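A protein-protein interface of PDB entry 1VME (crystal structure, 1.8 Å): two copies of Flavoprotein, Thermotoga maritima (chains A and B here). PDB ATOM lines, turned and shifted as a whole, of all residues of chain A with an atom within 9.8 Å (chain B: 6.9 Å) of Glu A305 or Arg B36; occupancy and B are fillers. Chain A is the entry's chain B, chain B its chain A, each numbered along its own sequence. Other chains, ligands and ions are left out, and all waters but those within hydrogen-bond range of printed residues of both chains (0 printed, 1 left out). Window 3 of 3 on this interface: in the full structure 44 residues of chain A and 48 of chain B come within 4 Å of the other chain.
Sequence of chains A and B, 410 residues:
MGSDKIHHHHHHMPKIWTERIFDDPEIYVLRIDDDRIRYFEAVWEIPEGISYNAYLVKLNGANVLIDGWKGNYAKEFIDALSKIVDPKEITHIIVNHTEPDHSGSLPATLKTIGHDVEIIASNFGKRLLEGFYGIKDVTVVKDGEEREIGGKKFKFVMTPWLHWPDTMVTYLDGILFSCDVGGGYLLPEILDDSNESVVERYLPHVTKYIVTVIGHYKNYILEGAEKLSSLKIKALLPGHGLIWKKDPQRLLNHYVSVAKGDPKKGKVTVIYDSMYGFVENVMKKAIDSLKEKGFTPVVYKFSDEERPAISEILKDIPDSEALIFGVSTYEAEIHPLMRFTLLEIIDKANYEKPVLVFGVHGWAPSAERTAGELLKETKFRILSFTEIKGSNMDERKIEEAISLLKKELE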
ATOM      1  N   SER A 274      18.517 -32.907   8.856  1.00  0.00           N
ATOM      2  CA  SER A 274      17.394 -32.641   7.968  1.00  0.00           C
ATOM      3  C   SER A 274      17.942 -31.882   6.806  1.00  0.00           C
ATOM      4  O   SER A 274      18.355 -30.747   6.940  1.00  0.00           O
ATOM      5  CB  SER A 274      16.241 -31.866   8.620  1.00  0.00           C
ATOM      6  OG  SER A 274      15.112 -31.794   7.711  1.00  0.00           O
ATOM      7  N   MET A 275      17.929 -32.538   5.669  1.00  0.00           N
ATOM      8  CA  MET A 275      18.422 -31.913   4.442  1.00  0.00           C
ATOM      9  C   MET A 275      17.383 -31.041   3.791  1.00  0.00           C
ATOM     10  O   MET A 275      17.650 -29.897   3.432  1.00  0.00           O
ATOM     11  CB  MET A 275      18.861 -32.997   3.521  1.00  0.00           C
ATOM     12  CG  MET A 275      19.959 -33.855   4.167  1.00  0.00           C
ATOM     13  SD  MET A 275      20.772 -35.095   2.907  1.00  0.00           S
ATOM     14  CE  MET A 275      20.668 -33.654   1.558  1.00  0.00           C
ATOM     15  N   TYR A 276      16.171 -31.546   3.654  1.00  0.00           N
ATOM     16  CA  TYR A 276      15.131 -30.802   2.963  1.00  0.00           C
ATOM     17  C   TYR A 276      13.819 -30.663   3.676  1.00  0.00           C
ATOM     18  O   TYR A 276      12.811 -30.311   3.078  1.00  0.00           O
ATOM     19  CB  TYR A 276      14.929 -31.491   1.625  1.00  0.00           C
ATOM     20  CG  TYR A 276      16.122 -31.293   0.768  1.00  0.00           C
ATOM     21  CD1 TYR A 276      16.475 -29.988   0.350  1.00  0.00           C
ATOM     22  CD2 TYR A 276      16.913 -32.361   0.380  1.00  0.00           C
ATOM     23  CE1 TYR A 276      17.587 -29.746  -0.456  1.00  0.00           C
ATOM     24  CE2 TYR A 276      18.019 -32.159  -0.411  1.00  0.00           C
ATOM     25  CZ  TYR A 276      18.385 -30.824  -0.853  1.00  0.00           C
ATOM     26  OH  TYR A 276      19.508 -30.509  -1.688  1.00  0.00           O
ATOM     27  N   LYS A 301      20.014 -30.351  15.949  1.00  0.00           N
ATOM     28  CA  LYS A 301      19.650 -30.470  14.521  1.00  0.00           C
ATOM     29  C   LYS A 301      20.806 -30.057  13.625  1.00  0.00           C
ATOM     30  O   LYS A 301      21.293 -28.928  13.745  1.00  0.00           O
ATOM     31  CB  LYS A 301      18.457 -29.518  14.257  1.00  0.00           C
ATOM     32  CG  LYS A 301      17.952 -29.455  12.808  1.00  0.00           C
ATOM     33  CD  LYS A 301      16.847 -28.368  12.619  1.00  0.00           C
ATOM     34  CE  LYS A 301      16.212 -28.457  11.183  1.00  0.00           C
ATOM     35  NZ  LYS A 301      15.137 -27.402  10.984  1.00  0.00           N
ATOM     36  N   PHE A 302      21.203 -30.937  12.709  1.00  0.00           N
ATOM     37  CA  PHE A 302      22.119 -30.603  11.641  1.00  0.00           C
ATOM     38  C   PHE A 302      21.244 -30.247  10.444  1.00  0.00           C
ATOM     39  O   PHE A 302      20.525 -31.130   9.909  1.00  0.00           O
ATOM     40  CB  PHE A 302      22.993 -31.783  11.276  1.00  0.00           C
ATOM     41  CG  PHE A 302      23.946 -32.202  12.362  1.00  0.00           C
ATOM     42  CD1 PHE A 302      25.195 -31.644  12.472  1.00  0.00           C
ATOM     43  CD2 PHE A 302      23.591 -33.168  13.263  1.00  0.00           C
ATOM     44  CE1 PHE A 302      26.051 -32.052  13.479  1.00  0.00           C
ATOM     45  CE2 PHE A 302      24.442 -33.575  14.253  1.00  0.00           C
ATOM     46  CZ  PHE A 302      25.649 -32.985  14.394  1.00  0.00           C
ATOM     47  N   SER A 303      21.300 -28.991  10.009  1.00  0.00           N
ATOM     48  CA  SER A 303      20.481 -28.530   8.903  1.00  0.00           C
ATOM     49  C   SER A 303      21.352 -27.751   7.925  1.00  0.00           C
ATOM     50  O   SER A 303      22.593 -27.675   8.092  1.00  0.00           O
ATOM     51  CB  SER A 303      19.351 -27.657   9.426  1.00  0.00           C
ATOM     52  OG  SER A 303      19.864 -26.399   9.771  1.00  0.00           O
ATOM     53  N   ASP A 304      20.736 -27.190   6.883  1.00  0.00           N
ATOM     54  CA  ASP A 304      21.538 -26.432   5.935  1.00  0.00           C
ATOM     55  C   ASP A 304      21.957 -25.025   6.435  1.00  0.00           C
ATOM     56  O   ASP A 304      22.701 -24.326   5.751  1.00  0.00           O
ATOM     57  CB  ASP A 304      20.937 -26.443   4.541  1.00  0.00           C
ATOM     58  CG  ASP A 304      19.605 -25.770   4.447  1.00  0.00           C
ATOM     59  OD1 ASP A 304      19.294 -24.976   5.369  1.00  0.00           O
ATOM     60  OD2 ASP A 304      18.875 -26.048   3.439  1.00  0.00           O
ATOM     61  N   GLU A 305      21.497 -24.646   7.633  1.00  0.00           N
ATOM     62  CA  GLU A 305      21.901 -23.412   8.297  1.00  0.00           C
ATOM     63  C   GLU A 305      22.536 -23.562   9.689  1.00  0.00           C
ATOM     64  O   GLU A 305      23.145 -22.617  10.166  1.00  0.00           O
ATOM     65  CB  GLU A 305      20.651 -22.540   8.466  1.00  0.00           C
ATOM     66  CG  GLU A 305      20.165 -22.029   7.161  1.00  0.00           C
ATOM     67  CD  GLU A 305      19.054 -21.010   7.311  1.00  0.00           C
ATOM     68  OE1 GLU A 305      18.630 -20.721   8.464  1.00  0.00           O
ATOM     69  OE2 GLU A 305      18.613 -20.502   6.265  1.00  0.00           O
ATOM     70  N   GLU A 306      22.393 -24.721  10.315  1.00  0.00           N
ATOM     71  CA  GLU A 306      22.779 -24.949  11.698  1.00  0.00           C
ATOM     72  C   GLU A 306      23.581 -26.223  11.858  1.00  0.00           C
ATOM     73  O   GLU A 306      23.297 -27.226  11.233  1.00  0.00           O
ATOM     74  CB  GLU A 306      21.532 -25.062  12.550  1.00  0.00           C
ATOM     75  CG  GLU A 306      20.900 -23.705  12.774  1.00  0.00           C
ATOM     76  CD  GLU A 306      19.637 -23.775  13.651  1.00  0.00           C
ATOM     77  OE1 GLU A 306      19.148 -24.902  13.968  1.00  0.00           O
ATOM     78  OE2 GLU A 306      19.152 -22.678  14.041  1.00  0.00           O
ATOM     79  N   ARG A 307      24.610 -26.152  12.687  1.00  0.00           N
ATOM     80  CA  ARG A 307      25.492 -27.296  12.945  1.00  0.00           C
ATOM     81  C   ARG A 307      25.900 -27.248  14.411  1.00  0.00           C
ATOM     82  O   ARG A 307      26.721 -26.410  14.809  1.00  0.00           O
ATOM     83  CB  ARG A 307      26.729 -27.171  12.088  1.00  0.00           C
ATOM     84  CG  ARG A 307      27.675 -28.325  12.330  1.00  0.00           C
ATOM     85  CD  ARG A 307      28.706 -28.370  11.325  1.00  0.00           C
ATOM     86  NE  ARG A 307      28.072 -28.626  10.059  1.00  0.00           N
ATOM     87  CZ  ARG A 307      28.731 -28.908   8.953  1.00  0.00           C
ATOM     88  NH1 ARG A 307      30.059 -29.011   8.938  1.00  0.00           N
ATOM     89  NH2 ARG A 307      28.035 -29.130   7.868  1.00  0.00           N
ATOM     90  N   PRO A 308      25.306 -28.095  15.233  1.00  0.00           N
ATOM     91  CA  PRO A 308      25.637 -28.136  16.671  1.00  0.00           C
ATOM     92  C   PRO A 308      27.095 -28.553  16.896  1.00  0.00           C
ATOM     93  O   PRO A 308      27.683 -29.222  16.057  1.00  0.00           O
ATOM     94  CB  PRO A 308      24.745 -29.263  17.207  1.00  0.00           C
ATOM     95  CG  PRO A 308      23.758 -29.511  16.143  1.00  0.00           C
ATOM     96  CD  PRO A 308      24.308 -29.104  14.854  1.00  0.00           C
ATOM     97  N   LEU A 337      27.486 -36.239   8.885  1.00  0.00           N
ATOM     98  CA  LEU A 337      27.488 -35.659  10.251  1.00  0.00           C
ATOM     99  C   LEU A 337      26.813 -36.564  11.256  1.00  0.00           C
ATOM    100  O   LEU A 337      27.202 -36.548  12.442  1.00  0.00           O
ATOM    101  CB  LEU A 337      26.899 -34.230  10.293  1.00  0.00           C
ATOM    102  CG  LEU A 337      27.696 -33.226   9.443  1.00  0.00           C
ATOM    103  CD1 LEU A 337      27.081 -31.863   9.595  1.00  0.00           C
ATOM    104  CD2 LEU A 337      29.145 -33.178   9.792  1.00  0.00           C
ATOM    105  N   HIS B  10      20.798 -11.297   7.826  1.00  0.00           N
ATOM    106  CA  HIS B  10      20.538 -10.843   6.464  1.00  0.00           C
ATOM    107  C   HIS B  10      19.719  -9.580   6.348  1.00  0.00           C
ATOM    108  O   HIS B  10      18.586  -9.526   6.797  1.00  0.00           O
ATOM    109  CB  HIS B  10      19.908 -11.955   5.635  1.00  0.00           C
ATOM    110  CG  HIS B  10      20.873 -13.049   5.357  1.00  0.00           C
ATOM    111  ND1 HIS B  10      20.955 -14.174   6.148  1.00  0.00           N
ATOM    112  CD2 HIS B  10      21.879 -13.136   4.458  1.00  0.00           C
ATOM    113  CE1 HIS B  10      21.945 -14.934   5.715  1.00  0.00           C
ATOM    114  NE2 HIS B  10      22.523 -14.325   4.693  1.00  0.00           N
ATOM    115  N   HIS B  11      20.296  -8.584   5.685  1.00  0.00           N
ATOM    116  CA  HIS B  11      19.666  -7.279   5.556  1.00  0.00           C
ATOM    117  C   HIS B  11      18.704  -7.161   4.376  1.00  0.00           C
ATOM    118  O   HIS B  11      17.897  -6.229   4.341  1.00  0.00           O
ATOM    119  CB  HIS B  11      20.750  -6.206   5.449  1.00  0.00           C
ATOM    120  CG  HIS B  11      21.636  -6.139   6.647  1.00  0.00           C
ATOM    121  ND1 HIS B  11      21.453  -5.216   7.658  1.00  0.00           N
ATOM    122  CD2 HIS B  11      22.690  -6.899   7.017  1.00  0.00           C
ATOM    123  CE1 HIS B  11      22.370  -5.403   8.590  1.00  0.00           C
ATOM    124  NE2 HIS B  11      23.130  -6.424   8.230  1.00  0.00           N
ATOM    125  N   HIS B  12      18.780  -8.089   3.417  1.00  0.00           N
ATOM    126  CA  HIS B  12      17.938  -8.039   2.222  1.00  0.00           C
ATOM    127  C   HIS B  12      17.422  -9.408   1.821  1.00  0.00           C
ATOM    128  O   HIS B  12      17.984 -10.424   2.219  1.00  0.00           O
ATOM    129  CB  HIS B  12      18.720  -7.436   1.056  1.00  0.00           C
ATOM    130  CG  HIS B  12      19.411  -6.147   1.398  1.00  0.00           C
ATOM    131  ND1 HIS B  12      18.731  -5.026   1.833  1.00  0.00           N
ATOM    132  CD2 HIS B  12      20.722  -5.806   1.378  1.00  0.00           C
ATOM    133  CE1 HIS B  12      19.593  -4.050   2.061  1.00  0.00           C
ATOM    134  NE2 HIS B  12      20.807  -4.497   1.789  1.00  0.00           N
ATOM    135  N   MET B  13      16.350  -9.399   1.037  1.00  0.00           N
ATOM    136  CA  MET B  13      15.774 -10.609   0.433  1.00  0.00           C
ATOM    137  C   MET B  13      16.769 -11.178  -0.558  1.00  0.00           C
ATOM    138  O   MET B  13      17.533 -10.422  -1.138  1.00  0.00           O
ATOM    139  CB  MET B  13      14.515 -10.282  -0.361  1.00  0.00           C
ATOM    140  CG  MET B  13      13.624  -9.204   0.220  1.00  0.00           C
ATOM    141  SD  MET B  13      12.225  -8.808  -1.039  1.00  0.00           S
ATOM    142  CE  MET B  13      13.305  -8.246  -2.643  1.00  0.00           C
ATOM    143  N   PRO B  14      16.755 -12.510  -0.779  1.00  0.00           N
ATOM    144  CA  PRO B  14      17.614 -13.048  -1.826  1.00  0.00           C
ATOM    145  C   PRO B  14      17.413 -12.398  -3.169  1.00  0.00           C
ATOM    146  O   PRO B  14      16.295 -12.086  -3.533  1.00  0.00           O
ATOM    147  CB  PRO B  14      17.176 -14.515  -1.920  1.00  0.00           C
ATOM    148  CG  PRO B  14      16.707 -14.818  -0.518  1.00  0.00           C
ATOM    149  CD  PRO B  14      16.017 -13.581  -0.078  1.00  0.00           C
ATOM    150  N   LYS B  15      18.509 -12.204  -3.887  1.00  0.00           N
ATOM    151  CA  LYS B  15      18.485 -11.635  -5.233  1.00  0.00           C
ATOM    152  C   LYS B  15      17.830 -12.585  -6.189  1.00  0.00           C
ATOM    153  O   LYS B  15      18.181 -13.767  -6.210  1.00  0.00           O
ATOM    154  CB  LYS B  15      19.901 -11.381  -5.750  1.00  0.00           C
ATOM    155  CG  LYS B  15      19.943 -10.641  -7.092  1.00  0.00           C
ATOM    156  CD  LYS B  15      21.383 -10.326  -7.491  1.00  0.00           C
ATOM    157  CE  LYS B  15      21.435  -9.266  -8.603  1.00  0.00           C
ATOM    158  NZ  LYS B  15      22.888  -8.943  -8.982  1.00  0.00           N
ATOM    159  N   ASP B  33      19.385 -16.459  -5.727  1.00  0.00           N
ATOM    160  CA  ASP B  33      20.712 -16.518  -5.176  1.00  0.00           C
ATOM    161  C   ASP B  33      20.575 -16.796  -3.679  1.00  0.00           C
ATOM    162  O   ASP B  33      20.248 -15.909  -2.916  1.00  0.00           O
ATOM    163  CB  ASP B  33      21.401 -15.187  -5.451  1.00  0.00           C
ATOM    164  CG  ASP B  33      21.930 -15.082  -6.893  1.00  0.00           C
ATOM    165  OD1 ASP B  33      21.710 -16.036  -7.669  1.00  0.00           O
ATOM    166  OD2 ASP B  33      22.534 -14.032  -7.232  1.00  0.00           O
ATOM    167  N   ASP B  34      20.828 -18.024  -3.290  1.00  0.00           N
ATOM    168  CA  ASP B  34      20.657 -18.440  -1.904  1.00  0.00           C
ATOM    169  C   ASP B  34      21.904 -18.096  -1.121  1.00  0.00           C
ATOM    170  O   ASP B  34      22.941 -18.831  -1.191  1.00  0.00           O
ATOM    171  CB  ASP B  34      20.391 -19.935  -1.842  1.00  0.00           C
ATOM    172  CG  ASP B  34      19.902 -20.407  -0.460  1.00  0.00           C
ATOM    173  OD1 ASP B  34      19.863 -19.578   0.481  1.00  0.00           O
ATOM    174  OD2 ASP B  34      19.491 -21.615  -0.341  1.00  0.00           O
ATOM    175  N   ASP B  35      21.816 -16.970  -0.427  1.00  0.00           N
ATOM    176  CA  ASP B  35      22.854 -16.510   0.485  1.00  0.00           C
ATOM    177  C   ASP B  35      22.464 -16.802   1.953  1.00  0.00           C
ATOM    178  O   ASP B  35      23.137 -16.353   2.873  1.00  0.00           O
ATOM    179  CB  ASP B  35      23.153 -15.028   0.259  1.00  0.00           C
ATOM    180  CG  ASP B  35      21.939 -14.149   0.439  1.00  0.00           C
ATOM    181  OD1 ASP B  35      20.838 -14.640   0.786  1.00  0.00           O
ATOM    182  OD2 ASP B  35      22.060 -12.937   0.182  1.00  0.00           O
ATOM    183  N   ARG B  36      21.362 -17.517   2.174  1.00  0.00           N
ATOM    184  CA  ARG B  36      20.921 -17.932   3.515  1.00  0.00           C
ATOM    185  C   ARG B  36      21.599 -19.257   3.887  1.00  0.00           C
ATOM    186  O   ARG B  36      22.071 -19.438   5.007  1.00  0.00           O
ATOM    187  CB  ARG B  36      19.424 -18.143   3.546  1.00  0.00           C
ATOM    188  CG  ARG B  36      18.618 -16.976   3.961  1.00  0.00           C
ATOM    189  CD  ARG B  36      18.733 -15.829   3.044  1.00  0.00           C
ATOM    190  NE  ARG B  36      17.898 -14.727   3.537  1.00  0.00           N
ATOM    191  CZ  ARG B  36      17.940 -13.481   3.078  1.00  0.00           C
ATOM    192  NH1 ARG B  36      18.771 -13.155   2.077  1.00  0.00           N
ATOM    193  NH2 ARG B  36      17.137 -12.564   3.626  1.00  0.00           N
ATOM    194  N   ILE B  37      21.621 -20.179   2.953  1.00  0.00           N
ATOM    195  CA  ILE B  37      22.238 -21.496   3.169  1.00  0.00           C
ATOM    196  C   ILE B  37      23.688 -21.396   3.586  1.00  0.00           C
ATOM    197  O   ILE B  37      24.441 -20.556   3.092  1.00  0.00           O
ATOM    198  CB  ILE B  37      22.034 -22.398   1.933  1.00  0.00           C
ATOM    199  CG1 ILE B  37      22.398 -23.859   2.172  1.00  0.00           C
ATOM    200  CG2 ILE B  37      22.804 -21.871   0.733  1.00  0.00           C
ATOM    201  CD1 ILE B  37      21.762 -24.783   1.171  1.00  0.00           C
ATOM    202  N   ARG B  38      24.087 -22.230   4.551  1.00  0.00           N
ATOM    203  CA  ARG B  38      25.445 -22.288   5.038  1.00  0.00           C
ATOM    204  C   ARG B  38      26.135 -23.597   4.695  1.00  0.00           C
ATOM    205  O   ARG B  38      27.345 -23.617   4.485  1.00  0.00           O
ATOM    206  CB  ARG B  38      25.485 -22.054   6.532  1.00  0.00           C
ATOM    207  CG  ARG B  38      24.961 -20.648   6.917  1.00  0.00           C
ATOM    208  CD  ARG B  38      25.102 -20.353   8.390  1.00  0.00           C
ATOM    209  NE  ARG B  38      26.502 -20.344   8.753  1.00  0.00           N
ATOM    210  CZ  ARG B  38      26.971 -20.526   9.987  1.00  0.00           C
ATOM    211  NH1 ARG B  38      26.143 -20.743  11.016  1.00  0.00           N
ATOM    212  NH2 ARG B  38      28.291 -20.501  10.176  1.00  0.00           N
ATOM    213  N   TYR B  39      25.362 -24.684   4.695  1.00  0.00           N
ATOM    214  CA  TYR B  39      25.880 -26.036   4.542  1.00  0.00           C
ATOM    215  C   TYR B  39      25.056 -26.752   3.491  1.00  0.00           C
ATOM    216  O   TYR B  39      23.903 -27.112   3.722  1.00  0.00           O
ATOM    217  CB  TYR B  39      25.818 -26.788   5.865  1.00  0.00           C
ATOM    218  CG  TYR B  39      26.420 -26.024   7.000  1.00  0.00           C
ATOM    219  CD1 TYR B  39      27.786 -25.856   7.099  1.00  0.00           C
ATOM    220  CD2 TYR B  39      25.629 -25.518   7.989  1.00  0.00           C
ATOM    221  CE1 TYR B  39      28.331 -25.122   8.156  1.00  0.00           C
ATOM    222  CE2 TYR B  39      26.151 -24.816   9.055  1.00  0.00           C
ATOM    223  CZ  TYR B  39      27.484 -24.620   9.130  1.00  0.00           C
ATOM    224  OH  TYR B  39      28.005 -23.919  10.145  1.00  0.00           O
ATOM    225  N   ALA B  42      23.250 -30.032   4.070  1.00  0.00           N
ATOM    226  CA  ALA B  42      23.478 -29.970   5.492  1.00  0.00           C
ATOM    227  C   ALA B  42      24.889 -30.419   5.928  1.00  0.00           C
ATOM    228  O   ALA B  42      25.089 -30.765   7.076  1.00  0.00           O
ATOM    229  CB  ALA B  42      22.368 -30.758   6.277  1.00  0.00           C
ATOM    230  N   GLY B  49      27.665 -19.279  -1.074  1.00  0.00           N
ATOM    231  CA  GLY B  49      26.280 -19.508  -1.507  1.00  0.00           C
ATOM    232  C   GLY B  49      26.173 -20.372  -2.737  1.00  0.00           C
ATOM    233  O   GLY B  49      27.175 -20.925  -3.273  1.00  0.00           O
ATOM    234  N   LYS B  70      14.198 -24.383  -4.497  1.00  0.00           N
ATOM    235  CA  LYS B  70      14.061 -24.981  -3.159  1.00  0.00           C
ATOM    236  C   LYS B  70      12.796 -24.509  -2.514  1.00  0.00           C
ATOM    237  O   LYS B  70      12.365 -23.369  -2.720  1.00  0.00           O
ATOM    238  CB  LYS B  70      15.288 -24.593  -2.312  1.00  0.00           C
ATOM    239  CG  LYS B  70      15.570 -25.356  -1.021  1.00  0.00           C
ATOM    240  CD  LYS B  70      16.937 -24.870  -0.519  1.00  0.00           C
ATOM    241  CE  LYS B  70      17.379 -25.436   0.816  1.00  0.00           C
ATOM    242  NZ  LYS B  70      17.018 -24.525   1.865  1.00  0.00           N
ATOM    243  N   ASN B  72      11.695 -23.623   0.425  1.00  0.00           N
ATOM    244  CA  ASN B  72      11.653 -22.423   1.263  1.00  0.00           C
ATOM    245  C   ASN B  72      11.504 -21.133   0.445  1.00  0.00           C
ATOM    246  O   ASN B  72      11.118 -20.109   0.970  1.00  0.00           O
ATOM    247  CB  ASN B  72      12.805 -22.346   2.270  1.00  0.00           C
ATOM    248  CG  ASN B  72      14.168 -22.298   1.627  1.00  0.00           C
ATOM    249  OD1 ASN B  72      14.455 -23.062   0.719  1.00  0.00           O
ATOM    250  ND2 ASN B  72      15.051 -21.417   2.142  1.00  0.00           N
ATOM    251  N   TYR B  73      11.726 -21.220  -0.859  1.00  0.00           N
ATOM    252  CA  TYR B  73      11.525 -20.102  -1.754  1.00  0.00           C
ATOM    253  C   TYR B  73      10.335 -20.322  -2.711  1.00  0.00           C
ATOM    254  O   TYR B  73      10.239 -19.662  -3.733  1.00  0.00           O
ATOM    255  CB  TYR B  73      12.806 -19.856  -2.516  1.00  0.00           C
ATOM    256  CG  TYR B  73      14.002 -19.511  -1.641  1.00  0.00           C
ATOM    257  CD1 TYR B  73      13.965 -18.400  -0.799  1.00  0.00           C
ATOM    258  CD2 TYR B  73      15.184 -20.275  -1.673  1.00  0.00           C
ATOM    259  CE1 TYR B  73      15.034 -18.048   0.010  1.00  0.00           C
ATOM    260  CE2 TYR B  73      16.286 -19.911  -0.868  1.00  0.00           C
ATOM    261  CZ  TYR B  73      16.198 -18.783  -0.028  1.00  0.00           C
ATOM    262  OH  TYR B  73      17.272 -18.422   0.796  1.00  0.00           O
ATOM    263  N   LEU B 187      27.732 -17.264  -6.241  1.00  0.00           N
ATOM    264  CA  LEU B 187      26.648 -16.405  -6.797  1.00  0.00           C
ATOM    265  C   LEU B 187      27.321 -15.446  -7.758  1.00  0.00           C
ATOM    266  O   LEU B 187      27.823 -14.403  -7.356  1.00  0.00           O
ATOM    267  CB  LEU B 187      25.916 -15.679  -5.687  1.00  0.00           C
ATOM    268  CG  LEU B 187      25.363 -16.606  -4.617  1.00  0.00           C
ATOM    269  CD1 LEU B 187      24.781 -15.840  -3.485  1.00  0.00           C
ATOM    270  CD2 LEU B 187      24.354 -17.573  -5.206  1.00  0.00           C
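No position is printed for both chains.
OD2 of Asp A304 lies within salt-bridge range of NZ of Lys B70, 2.9 Å away.
The backbone carbonyl oxygen (O) of Ala B42 is in hydrogen-bond range of the guanidinium group (NH2) of Arg A307, at 3.5 Å.
The backbone carbonyl oxygen of Asp A304 lies within hydrogen-bond range of the backbone NH of Arg B38, at 2.8 Å.
The backbone carbonyl oxygen of Asp A304 sits at hydrogen-bond distance from the backbone NH of Tyr B39, at 2.9 Å.
Printed residues of chain B within 4 Å of Glu A305: Arg B36 (3.7 Å), Arg B38 (3.5 Å) and Tyr B39 (3.9 Å).
Printed residues of chain A within 4 Å of Arg B36: Glu A305 (3.7 Å).
No residue of chain A comes within 4 Å of Asp B35.
Printed residues of chain B within 4 Å of Leu A337: Ala B42 (3.4 Å).
Printed residues of chain B within 4 Å of Glu A306: Tyr B39.
Of the printed residues of chain B, Asp A304 touches Ile B37 (3.6 Å), Arg B38 (2.8 Å), Tyr B39 (2.9 Å), Ala B42 (3.97 Å) and Lys B70 (2.9 Å).
Printed residues of chain A within 4 Å of Lys B70: Asp A304 (2.9 Å).
Printed residues of chain A within 4 Å of Arg B38: Asp A304 and Glu A305.
Phe A302 touches none of the printed residues of chain B.
Ser A274 touches none of the printed residues of chain B.
The nearest residue of chain B that does not touch Glu A305 is Ile B37 (4.5 Å).
The nearest residue of chain A that does not touch Arg B36 is Asp A304 (5.0 Å).
Among the printed residues, merely in contact across the chains: Ser A303 with Tyr B39, Ser A303 with Ala B42, Asp A304 with Ile B37, Asp A304 with Ala B42, Glu A305 with Arg B36, Glu A305 with Arg B38, Glu A305 with Tyr B39, Glu A306 with Tyr B39, Arg A307 with Tyr B39 and Leu A337 with Ala B42.
The side-chain amide oxygen (OD1) of Asn B72 lies close to the side-chain amino group (NZ) of Lys B70 (3.2 Å).
O of His B12 sits at hydrogen-bond distance from NH2 of Arg B36, 2.7 Å away.
OD1 of Asp B34 lies within hydrogen-bond range of N of Ile B37, at 3.1 Å.
The side-chain hydroxyl of Ser A303 sits at hydrogen-bond distance from the backbone NH of Glu A306 (3.1 Å).
The guanidinium group (NH2) of Arg B38 sits at hydrogen-bond distance from the side-chain hydroxyl (OH) of Tyr B39 (3.4 Å).
The side-chain carboxylate of Asp B35 lies within salt-bridge range of the guanidinium group of Arg B36, 2.9 Å away.
Hydrophobic or aromatic side chains of chain B within 4 Å of the printed part of chain A: Ile B37, Tyr B39 and Ala B42.
Hydrophobic or aromatic side chains of chain A that line the printed part of chain B: Leu A337.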
